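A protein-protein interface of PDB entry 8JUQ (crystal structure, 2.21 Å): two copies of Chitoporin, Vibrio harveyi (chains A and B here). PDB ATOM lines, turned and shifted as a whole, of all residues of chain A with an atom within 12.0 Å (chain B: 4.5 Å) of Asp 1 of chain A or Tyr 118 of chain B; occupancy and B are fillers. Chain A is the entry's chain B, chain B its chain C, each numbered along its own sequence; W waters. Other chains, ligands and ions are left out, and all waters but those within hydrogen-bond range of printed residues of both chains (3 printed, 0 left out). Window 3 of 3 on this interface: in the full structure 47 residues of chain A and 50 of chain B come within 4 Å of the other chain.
O of Asp 1 of chain A is in hydrogen-bond range of OH of Tyr 79 of chain B, 3.1 Å away. The side-chain carboxylate (OD1) of Asp 1 of chain A is in salt-bridge range of the guanidinium group (NH1) of Arg 94 of chain B, at 3.3 Å. The backbone NH of Asp 1 of chain A sits at hydrogen-bond distance from the side-chain hydroxyl of Tyr 118 of chain B (3.0 Å). N of Asp 1 of chain A lies within hydrogen-bond range of OD1 of Asp 122 of chain B (3.0 Å). The side-chain carboxylate of Asp 1 of chain A is in salt-bridge range of the guanidinium group of Arg 148 of chain B (3.1 Å). The side-chain hydroxyl (OH) of Tyr 79 of chain B sits close to the backbone NH (N) of Gly 2 of chain A. OG of Ser 5 of chain A sits at hydrogen-bond distance from OD1 of Asp 122 of chain B (2.8 Å). The side-chain carboxylate of Asp 6 of chain A lies within salt-bridge range of the guanidinium group of Arg 94 of chain B (3.6 Å).
The side-chain amino group (NZ) of Lys 9 of chain A lies within salt-bridge range of the side-chain carboxylate (OD2) of Asp 6 of chain A (3.5 Å). The guanidinium group (NH1) of Arg 94 of chain B lies within hydrogen-bond range of the side-chain hydroxyl (OH) of Tyr 79 of chain B. OG1 of Thr 115 of chain B sits at hydrogen-bond distance from N of Tyr 118 of chain B, at 3.1 Å. The side-chain hydroxyl (OH) of Tyr 118 of chain B lies within hydrogen-bond range of the side-chain carboxylate (OD2) of Asp 135 of chain B, at 2.7 Å.
Of chain B, only Tyr 79, Arg 94, Tyr 118, Asp 122 and Arg 148 come within 4 Å of Asp 1 of chain A. Ala 3 of chain A touches none of the printed residues of chain B. Of the printed residues of chain B, Ser 5 of chain A touches Asp 122 (2.8 Å). Ala 8 of chain A touches none of the printed residues of chain B. Printed residues of chain A within 4 Å of Tyr 79 of chain B: Asp 1 and Gly 2. Of the printed residues of chain A, Arg 94 of chain B touches Asp 1 (3.3 Å) and Asp 6 (3.6 Å). No residue of chain A comes within 4 Å of Leu 114 of chain B. No residue of chain A comes within 4 Å of Pro 116 of chain B. No residue of chain A comes within 4 Å of Met 117 of chain B. No residue of chain A comes within 4 Å of Glu 119 of chain B. No residue of chain A comes within 4 Å of Leu 120 of chain B. No residue of chain A comes within 4 Å of Val 121 of chain B. Asp 122 of chain B touches just these residues of chain A: Asp 1 (3.0 Å) and Ser 5 (2.8 Å). No residue of chain A comes within 4 Å of Asp 135 of chain B. No residue of chain A comes within 4 Å of Tyr 145 of chain B. No residue of chain A comes within 4 Å of Asp 147 of chain B. Of the printed residues of chain A, Arg 148 of chain B touches Asp 1. The nearest residue of chain B that does not touch Asp 1 of chain A is Asp 135 of chain B (4.2 Å).
Hydrophobic or aromatic side chains of chain B within 4 Å of the printed part of chain A: Tyr 79 and Tyr 118. Printed residues of chain A that touch a printed residue of chain B: Asp 1, Gly 2, Ser 5 and Asp 6. Among the printed residues, 8 pairs touch across the chains.
No position is printed for both chains.
Water W3 lies within hydrogen-bond range of the side-chain carboxylate (OD2) of Asp 1 of chain A (2.5 Å), the guanidinium group (NH1) of Arg 94 of chain B (2.8 Å) and the guanidinium group (NH1) of Arg 148 of chain B (3.5 Å). Water W1 lies within hydrogen-bond range of the backbone carbonyl oxygen (O) of Ser 5 of chain A (2.7 Å), the side-chain hydroxyl (OH) of Tyr 79 of chain B (2.8 Å) and the backbone carbonyl oxygen (O) of Asp 1 of chain A (3.3 Å). Water W2 bridges OD2 of Asp 6 of chain A (2.9 Å) and NH2 of Arg 148 of chain B (3.0 Å).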
ATOM      1  N   ASP A   1      19.043  18.303  -2.229  1.00  0.00           N
ATOM      2  CA  ASP A   1      17.587  18.083  -2.276  1.00  0.00           C
ATOM      3  C   ASP A   1      17.307  16.590  -2.273  1.00  0.00           C
ATOM      4  O   ASP A   1      18.245  15.790  -2.391  1.00  0.00           O
ATOM      5  CB  ASP A   1      16.976  18.729  -3.528  1.00  0.00           C
ATOM      6  CG  ASP A   1      17.769  18.397  -4.814  1.00  0.00           C
ATOM      7  OD1 ASP A   1      18.964  18.040  -4.706  1.00  0.00           O
ATOM      8  OD2 ASP A   1      17.207  18.505  -5.925  1.00  0.00           O
ATOM      9  N   GLY A   2      16.030  16.213  -2.132  1.00  0.00           N
ATOM     10  CA  GLY A   2      15.623  14.830  -2.264  1.00  0.00           C
ATOM     11  C   GLY A   2      15.645  14.082  -0.940  1.00  0.00           C
ATOM     12  O   GLY A   2      16.190  14.534   0.065  1.00  0.00           O
ATOM     13  N   ALA A   3      15.085  12.873  -0.972  1.00  0.00           N
ATOM     14  CA  ALA A   3      14.962  12.071   0.239  1.00  0.00           C
ATOM     15  C   ALA A   3      16.306  11.805   0.921  1.00  0.00           C
ATOM     16  O   ALA A   3      16.364  11.749   2.154  1.00  0.00           O
ATOM     17  CB  ALA A   3      14.260  10.754  -0.096  1.00  0.00           C
ATOM     18  N   ASN A   4      17.401  11.682   0.163  1.00  0.00           N
ATOM     19  CA  ASN A   4      18.677  11.413   0.823  1.00  0.00           C
ATOM     20  C   ASN A   4      19.841  12.184   0.184  1.00  0.00           C
ATOM     21  O   ASN A   4      20.986  11.708   0.195  1.00  0.00           O
ATOM     22  CB  ASN A   4      18.987   9.912   0.845  1.00  0.00           C
ATOM     23  CG  ASN A   4      17.997   9.110   1.704  1.00  0.00           C
ATOM     24  OD1 ASN A   4      18.030   9.168   2.949  1.00  0.00           O
ATOM     25  ND2 ASN A   4      17.140   8.328   1.045  1.00  0.00           N
ATOM     26  N   SER A   5      19.560  13.366  -0.381  1.00  0.00           N
ATOM     27  CA  SER A   5      20.566  14.202  -1.032  1.00  0.00           C
ATOM     28  C   SER A   5      21.345  13.359  -2.025  1.00  0.00           C
ATOM     29  O   SER A   5      20.753  12.562  -2.756  1.00  0.00           O
ATOM     30  CB  SER A   5      21.503  14.851  -0.012  1.00  0.00           C
ATOM     31  OG  SER A   5      20.773  15.279   1.130  1.00  0.00           O
ATOM     32  N   ASP A   6      22.662  13.548  -2.080  1.00  0.00           N
ATOM     33  CA  ASP A   6      23.544  12.694  -2.863  1.00  0.00           C
ATOM     34  C   ASP A   6      24.292  11.686  -1.988  1.00  0.00           C
ATOM     35  O   ASP A   6      25.398  11.255  -2.341  1.00  0.00           O
ATOM     36  CB  ASP A   6      24.516  13.538  -3.691  1.00  0.00           C
ATOM     37  CG  ASP A   6      24.215  13.476  -5.200  1.00  0.00           C
ATOM     38  OD1 ASP A   6      23.564  12.503  -5.670  1.00  0.00           O
ATOM     39  OD2 ASP A   6      24.640  14.398  -5.927  1.00  0.00           O
ATOM     40  N   ALA A   7      23.692  11.287  -0.858  1.00  0.00           N
ATOM     41  CA  ALA A   7      24.377  10.388   0.068  1.00  0.00           C
ATOM     42  C   ALA A   7      24.676   9.040  -0.575  1.00  0.00           C
ATOM     43  O   ALA A   7      25.729   8.448  -0.312  1.00  0.00           O
ATOM     44  CB  ALA A   7      23.552  10.191   1.340  1.00  0.00           C
ATOM     45  N   ALA A   8      23.772   8.540  -1.418  1.00  0.00           N
ATOM     46  CA  ALA A   8      24.037   7.271  -2.083  1.00  0.00           C
ATOM     47  C   ALA A   8      25.355   7.329  -2.850  1.00  0.00           C
ATOM     48  O   ALA A   8      26.181   6.413  -2.764  1.00  0.00           O
ATOM     49  CB  ALA A   8      22.869   6.905  -2.998  1.00  0.00           C
ATOM     50  N   LYS A   9      25.593   8.436  -3.553  1.00  0.00           N
ATOM     51  CA  LYS A   9      26.804   8.601  -4.348  1.00  0.00           C
ATOM     52  C   LYS A   9      28.051   8.682  -3.471  1.00  0.00           C
ATOM     53  O   LYS A   9      29.144   8.330  -3.924  1.00  0.00           O
ATOM     54  CB  LYS A   9      26.665   9.860  -5.220  1.00  0.00           C
ATOM     55  CG  LYS A   9      27.177   9.770  -6.653  1.00  0.00           C
ATOM     56  CD  LYS A   9      27.335  11.195  -7.299  1.00  0.00           C
ATOM     57  CE  LYS A   9      26.184  11.614  -8.251  1.00  0.00           C
ATOM     58  NZ  LYS A   9      26.294  13.079  -8.738  1.00  0.00           N
ATOM     59  N   GLU A  10      27.919   9.168  -2.231  1.00  0.00           N
ATOM     60  CA  GLU A  10      29.045   9.323  -1.311  1.00  0.00           C
ATOM     61  C   GLU A  10      29.321   8.090  -0.455  1.00  0.00           C
ATOM     62  O   GLU A  10      30.479   7.842  -0.110  1.00  0.00           O
ATOM     63  CB  GLU A  10      28.810  10.531  -0.395  1.00  0.00           C
ATOM     64  N   TYR B  79      15.312  14.289 -11.483  1.00  0.00           N
ATOM     65  CA  TYR B  79      14.436  13.253 -10.937  1.00  0.00           C
ATOM     66  C   TYR B  79      13.394  12.829 -11.975  1.00  0.00           C
ATOM     67  O   TYR B  79      12.689  13.663 -12.531  1.00  0.00           O
ATOM     68  CB  TYR B  79      13.737  13.796  -9.693  1.00  0.00           C
ATOM     69  CG  TYR B  79      14.636  14.123  -8.521  1.00  0.00           C
ATOM     70  CD1 TYR B  79      15.838  13.440  -8.315  1.00  0.00           C
ATOM     71  CD2 TYR B  79      14.274  15.102  -7.605  1.00  0.00           C
ATOM     72  CE1 TYR B  79      16.653  13.736  -7.227  1.00  0.00           C
ATOM     73  CE2 TYR B  79      15.079  15.394  -6.491  1.00  0.00           C
ATOM     74  CZ  TYR B  79      16.259  14.709  -6.301  1.00  0.00           C
ATOM     75  OH  TYR B  79      17.058  15.012  -5.193  1.00  0.00           O
ATOM     76  N   ARG B  94      20.483  18.211 -13.011  1.00  0.00           N
ATOM     77  CA  ARG B  94      21.265  18.099 -11.787  1.00  0.00           C
ATOM     78  C   ARG B  94      22.714  18.513 -12.091  1.00  0.00           C
ATOM     79  O   ARG B  94      22.946  19.288 -13.009  1.00  0.00           O
ATOM     80  CB  ARG B  94      21.093  16.689 -11.193  1.00  0.00           C
ATOM     81  CG  ARG B  94      19.672  16.523 -10.572  1.00  0.00           C
ATOM     82  CD  ARG B  94      19.377  15.144  -9.933  1.00  0.00           C
ATOM     83  NE  ARG B  94      20.297  14.823  -8.845  1.00  0.00           N
ATOM     84  CZ  ARG B  94      20.143  15.198  -7.583  1.00  0.00           C
ATOM     85  NH1 ARG B  94      19.096  15.908  -7.193  1.00  0.00           N
ATOM     86  NH2 ARG B  94      21.053  14.825  -6.688  1.00  0.00           N
ATOM     87  N   LEU B 114      26.397  22.498  -6.695  1.00  0.00           N
ATOM     88  CA  LEU B 114      25.923  23.013  -5.412  1.00  0.00           C
ATOM     89  C   LEU B 114      26.841  24.133  -4.958  1.00  0.00           C
ATOM     90  O   LEU B 114      28.062  24.027  -5.089  1.00  0.00           O
ATOM     91  CB  LEU B 114      25.905  21.919  -4.340  1.00  0.00           C
ATOM     92  CG  LEU B 114      25.141  20.621  -4.660  1.00  0.00           C
ATOM     93  CD1 LEU B 114      25.164  19.640  -3.489  1.00  0.00           C
ATOM     94  CD2 LEU B 114      23.708  20.946  -5.086  1.00  0.00           C
ATOM     95  N   THR B 115      26.261  25.192  -4.381  1.00  0.00           N
ATOM     96  CA  THR B 115      27.092  26.202  -3.751  1.00  0.00           C
ATOM     97  C   THR B 115      27.762  25.618  -2.510  1.00  0.00           C
ATOM     98  O   THR B 115      27.295  24.620  -1.952  1.00  0.00           O
ATOM     99  CB  THR B 115      26.281  27.447  -3.367  1.00  0.00           C
ATOM    100  OG1 THR B 115      25.509  27.198  -2.178  1.00  0.00           O
ATOM    101  CG2 THR B 115      25.347  27.876  -4.519  1.00  0.00           C
ATOM    102  N   PRO B 116      28.898  26.198  -2.091  1.00  0.00           N
ATOM    103  CA  PRO B 116      29.582  25.696  -0.878  1.00  0.00           C
ATOM    104  C   PRO B 116      28.695  25.686   0.349  1.00  0.00           C
ATOM    105  O   PRO B 116      28.751  24.752   1.158  1.00  0.00           O
ATOM    106  CB  PRO B 116      30.761  26.678  -0.712  1.00  0.00           C
ATOM    107  CG  PRO B 116      31.055  27.139  -2.123  1.00  0.00           C
ATOM    108  CD  PRO B 116      29.673  27.253  -2.772  1.00  0.00           C
ATOM    109  N   MET B 117      27.880  26.723   0.521  1.00  0.00           N
ATOM    110  CA  MET B 117      26.982  26.784   1.663  1.00  0.00           C
ATOM    111  C   MET B 117      25.890  25.713   1.573  1.00  0.00           C
ATOM    112  O   MET B 117      25.625  24.986   2.543  1.00  0.00           O
ATOM    113  CB  MET B 117      26.378  28.181   1.741  1.00  0.00           C
ATOM    114  CG  MET B 117      24.998  28.215   2.384  1.00  0.00           C
ATOM    115  SD  MET B 117      25.147  28.267   4.169  1.00  0.00           S
ATOM    116  CE  MET B 117      25.970  29.831   4.462  1.00  0.00           C
ATOM    117  N   TYR B 118      25.252  25.599   0.407  1.00  0.00           N
ATOM    118  CA  TYR B 118      24.124  24.695   0.271  1.00  0.00           C
ATOM    119  C   TYR B 118      24.533  23.245   0.497  1.00  0.00           C
ATOM    120  O   TYR B 118      23.748  22.442   1.017  1.00  0.00           O
ATOM    121  CB  TYR B 118      23.497  24.818  -1.114  1.00  0.00           C
ATOM    122  CG  TYR B 118      22.362  23.834  -1.225  1.00  0.00           C
ATOM    123  CD1 TYR B 118      21.201  24.027  -0.476  1.00  0.00           C
ATOM    124  CD2 TYR B 118      22.466  22.685  -2.018  1.00  0.00           C
ATOM    125  CE1 TYR B 118      20.154  23.134  -0.524  1.00  0.00           C
ATOM    126  CE2 TYR B 118      21.421  21.767  -2.072  1.00  0.00           C
ATOM    127  CZ  TYR B 118      20.262  22.005  -1.313  1.00  0.00           C
ATOM    128  OH  TYR B 118      19.209  21.134  -1.333  1.00  0.00           O
ATOM    129  N   GLU B 119      25.753  22.893   0.110  1.00  0.00           N
ATOM    130  CA  GLU B 119      26.208  21.521   0.273  1.00  0.00           C
ATOM    131  C   GLU B 119      26.173  21.078   1.730  1.00  0.00           C
ATOM    132  O   GLU B 119      25.831  19.923   2.027  1.00  0.00           O
ATOM    133  CB  GLU B 119      27.611  21.390  -0.310  1.00  0.00           C
ATOM    134  CG  GLU B 119      28.075  19.965  -0.455  1.00  0.00           C
ATOM    135  CD  GLU B 119      29.475  19.924  -1.034  1.00  0.00           C
ATOM    136  OE1 GLU B 119      29.601  20.030  -2.275  1.00  0.00           O
ATOM    137  OE2 GLU B 119      30.442  19.833  -0.241  1.00  0.00           O
ATOM    138  N   LEU B 120      26.541  21.974   2.652  1.00  0.00           N
ATOM    139  CA  LEU B 120      26.481  21.663   4.075  1.00  0.00           C
ATOM    140  C   LEU B 120      25.055  21.675   4.597  1.00  0.00           C
ATOM    141  O   LEU B 120      24.720  20.893   5.496  1.00  0.00           O
ATOM    142  CB  LEU B 120      27.331  22.641   4.858  1.00  0.00           C
ATOM    143  CG  LEU B 120      28.796  22.297   4.668  1.00  0.00           C
ATOM    144  CD1 LEU B 120      29.641  23.534   4.925  1.00  0.00           C
ATOM    145  CD2 LEU B 120      29.145  21.140   5.614  1.00  0.00           C
ATOM    146  N   VAL B 121      24.213  22.574   4.073  1.00  0.00           N
ATOM    147  CA  VAL B 121      22.801  22.611   4.458  1.00  0.00           C
ATOM    148  C   VAL B 121      22.129  21.310   4.063  1.00  0.00           C
ATOM    149  O   VAL B 121      21.297  20.766   4.801  1.00  0.00           O
ATOM    150  CB  VAL B 121      22.093  23.810   3.790  1.00  0.00           C
ATOM    151  CG1 VAL B 121      20.562  23.690   3.924  1.00  0.00           C
ATOM    152  CG2 VAL B 121      22.594  25.133   4.342  1.00  0.00           C
ATOM    153  N   ASP B 122      22.470  20.808   2.876  1.00  0.00           N
ATOM    154  CA  ASP B 122      21.845  19.609   2.332  1.00  0.00           C
ATOM    155  C   ASP B 122      22.274  18.370   3.113  1.00  0.00           C
ATOM    156  O   ASP B 122      21.439  17.638   3.657  1.00  0.00           O
ATOM    157  CB  ASP B 122      22.236  19.494   0.852  1.00  0.00           C
ATOM    158  CG  ASP B 122      21.654  18.284   0.170  1.00  0.00           C
ATOM    159  OD1 ASP B 122      20.460  17.972   0.368  1.00  0.00           O
ATOM    160  OD2 ASP B 122      22.400  17.669  -0.615  1.00  0.00           O
ATOM    161  N   ASP B 135      16.231  23.380   4.681  1.00  0.00           N
ATOM    162  CA  ASP B 135      16.824  23.563   3.350  1.00  0.00           C
ATOM    163  C   ASP B 135      16.149  24.724   2.620  1.00  0.00           C
ATOM    164  O   ASP B 135      16.753  25.788   2.446  1.00  0.00           O
ATOM    165  CB  ASP B 135      16.773  22.233   2.589  1.00  0.00           C
ATOM    166  CG  ASP B 135      17.114  22.364   1.115  1.00  0.00           C
ATOM    167  OD1 ASP B 135      17.341  23.493   0.619  1.00  0.00           O
ATOM    168  OD2 ASP B 135      17.223  21.306   0.446  1.00  0.00           O
ATOM    169  N   TYR B 145      20.268  31.686   0.146  1.00  0.00           N
ATOM    170  CA  TYR B 145      21.389  31.085  -0.546  1.00  0.00           C
ATOM    171  C   TYR B 145      20.800  30.432  -1.779  1.00  0.00           C
ATOM    172  O   TYR B 145      19.603  30.155  -1.833  1.00  0.00           O
ATOM    173  CB  TYR B 145      22.154  30.063   0.321  1.00  0.00           C
ATOM    174  CG  TYR B 145      21.277  29.212   1.206  1.00  0.00           C
ATOM    175  CD1 TYR B 145      20.558  28.132   0.690  1.00  0.00           C
ATOM    176  CD2 TYR B 145      21.169  29.490   2.556  1.00  0.00           C
ATOM    177  CE1 TYR B 145      19.751  27.352   1.510  1.00  0.00           C
ATOM    178  CE2 TYR B 145      20.387  28.716   3.380  1.00  0.00           C
ATOM    179  CZ  TYR B 145      19.677  27.655   2.865  1.00  0.00           C
ATOM    180  OH  TYR B 145      18.886  26.930   3.725  1.00  0.00           O
ATOM    181  N   GLN B 146      21.635  30.237  -2.777  1.00  0.00           N
ATOM    182  CA  GLN B 146      21.262  29.348  -3.862  1.00  0.00           C
ATOM    183  C   GLN B 146      21.498  27.906  -3.413  1.00  0.00           C
ATOM    184  O   GLN B 146      22.140  27.656  -2.390  1.00  0.00           O
ATOM    185  CB  GLN B 146      22.069  29.688  -5.106  1.00  0.00           C
ATOM    186  CG  GLN B 146      22.037  31.183  -5.473  1.00  0.00           C
ATOM    187  CD  GLN B 146      20.621  31.677  -5.749  1.00  0.00           C
ATOM    188  OE1 GLN B 146      19.759  30.927  -6.216  1.00  0.00           O
ATOM    189  NE2 GLN B 146      20.370  32.937  -5.435  1.00  0.00           N
ATOM    190  N   ASP B 147      20.956  26.942  -4.158  1.00  0.00           N
ATOM    191  CA  ASP B 147      21.194  25.543  -3.826  1.00  0.00           C
ATOM    192  C   ASP B 147      22.013  24.912  -4.942  1.00  0.00           C
ATOM    193  O   ASP B 147      23.253  24.974  -4.905  1.00  0.00           O
ATOM    194  CB  ASP B 147      19.901  24.775  -3.496  1.00  0.00           C
ATOM    195  CG  ASP B 147      18.716  25.140  -4.361  1.00  0.00           C
ATOM    196  OD1 ASP B 147      18.757  24.999  -5.601  1.00  0.00           O
ATOM    197  OD2 ASP B 147      17.677  25.490  -3.770  1.00  0.00           O
ATOM    198  N   ARG B 148      21.397  24.287  -5.931  1.00  0.00           N
ATOM    199  CA  ARG B 148      22.118  23.855  -7.111  1.00  0.00           C
ATOM    200  C   ARG B 148      21.980  24.970  -8.129  1.00  0.00           C
ATOM    201  O   ARG B 148      20.868  25.409  -8.411  1.00  0.00           O
ATOM    202  CB  ARG B 148      21.566  22.534  -7.646  1.00  0.00           C
ATOM    203  CG  ARG B 148      22.321  21.967  -8.814  1.00  0.00           C
ATOM    204  CD  ARG B 148      21.748  20.575  -9.245  1.00  0.00           C
ATOM    205  NE  ARG B 148      22.029  19.586  -8.221  1.00  0.00           N
ATOM    206  CZ  ARG B 148      21.138  19.138  -7.348  1.00  0.00           C
ATOM    207  NH1 ARG B 148      19.861  19.505  -7.406  1.00  0.00           N
ATOM    208  NH2 ARG B 148      21.545  18.344  -6.364  1.00  0.00           N
HETATM  209  O   HOH W   1      18.457  12.910  -4.045  1.00  0.00           O
HETATM  210  O   HOH W   2      24.308  17.193  -6.476  1.00  0.00           O
HETATM  211  O   HOH W   3      17.065  17.613  -8.221  1.00  0.00           O
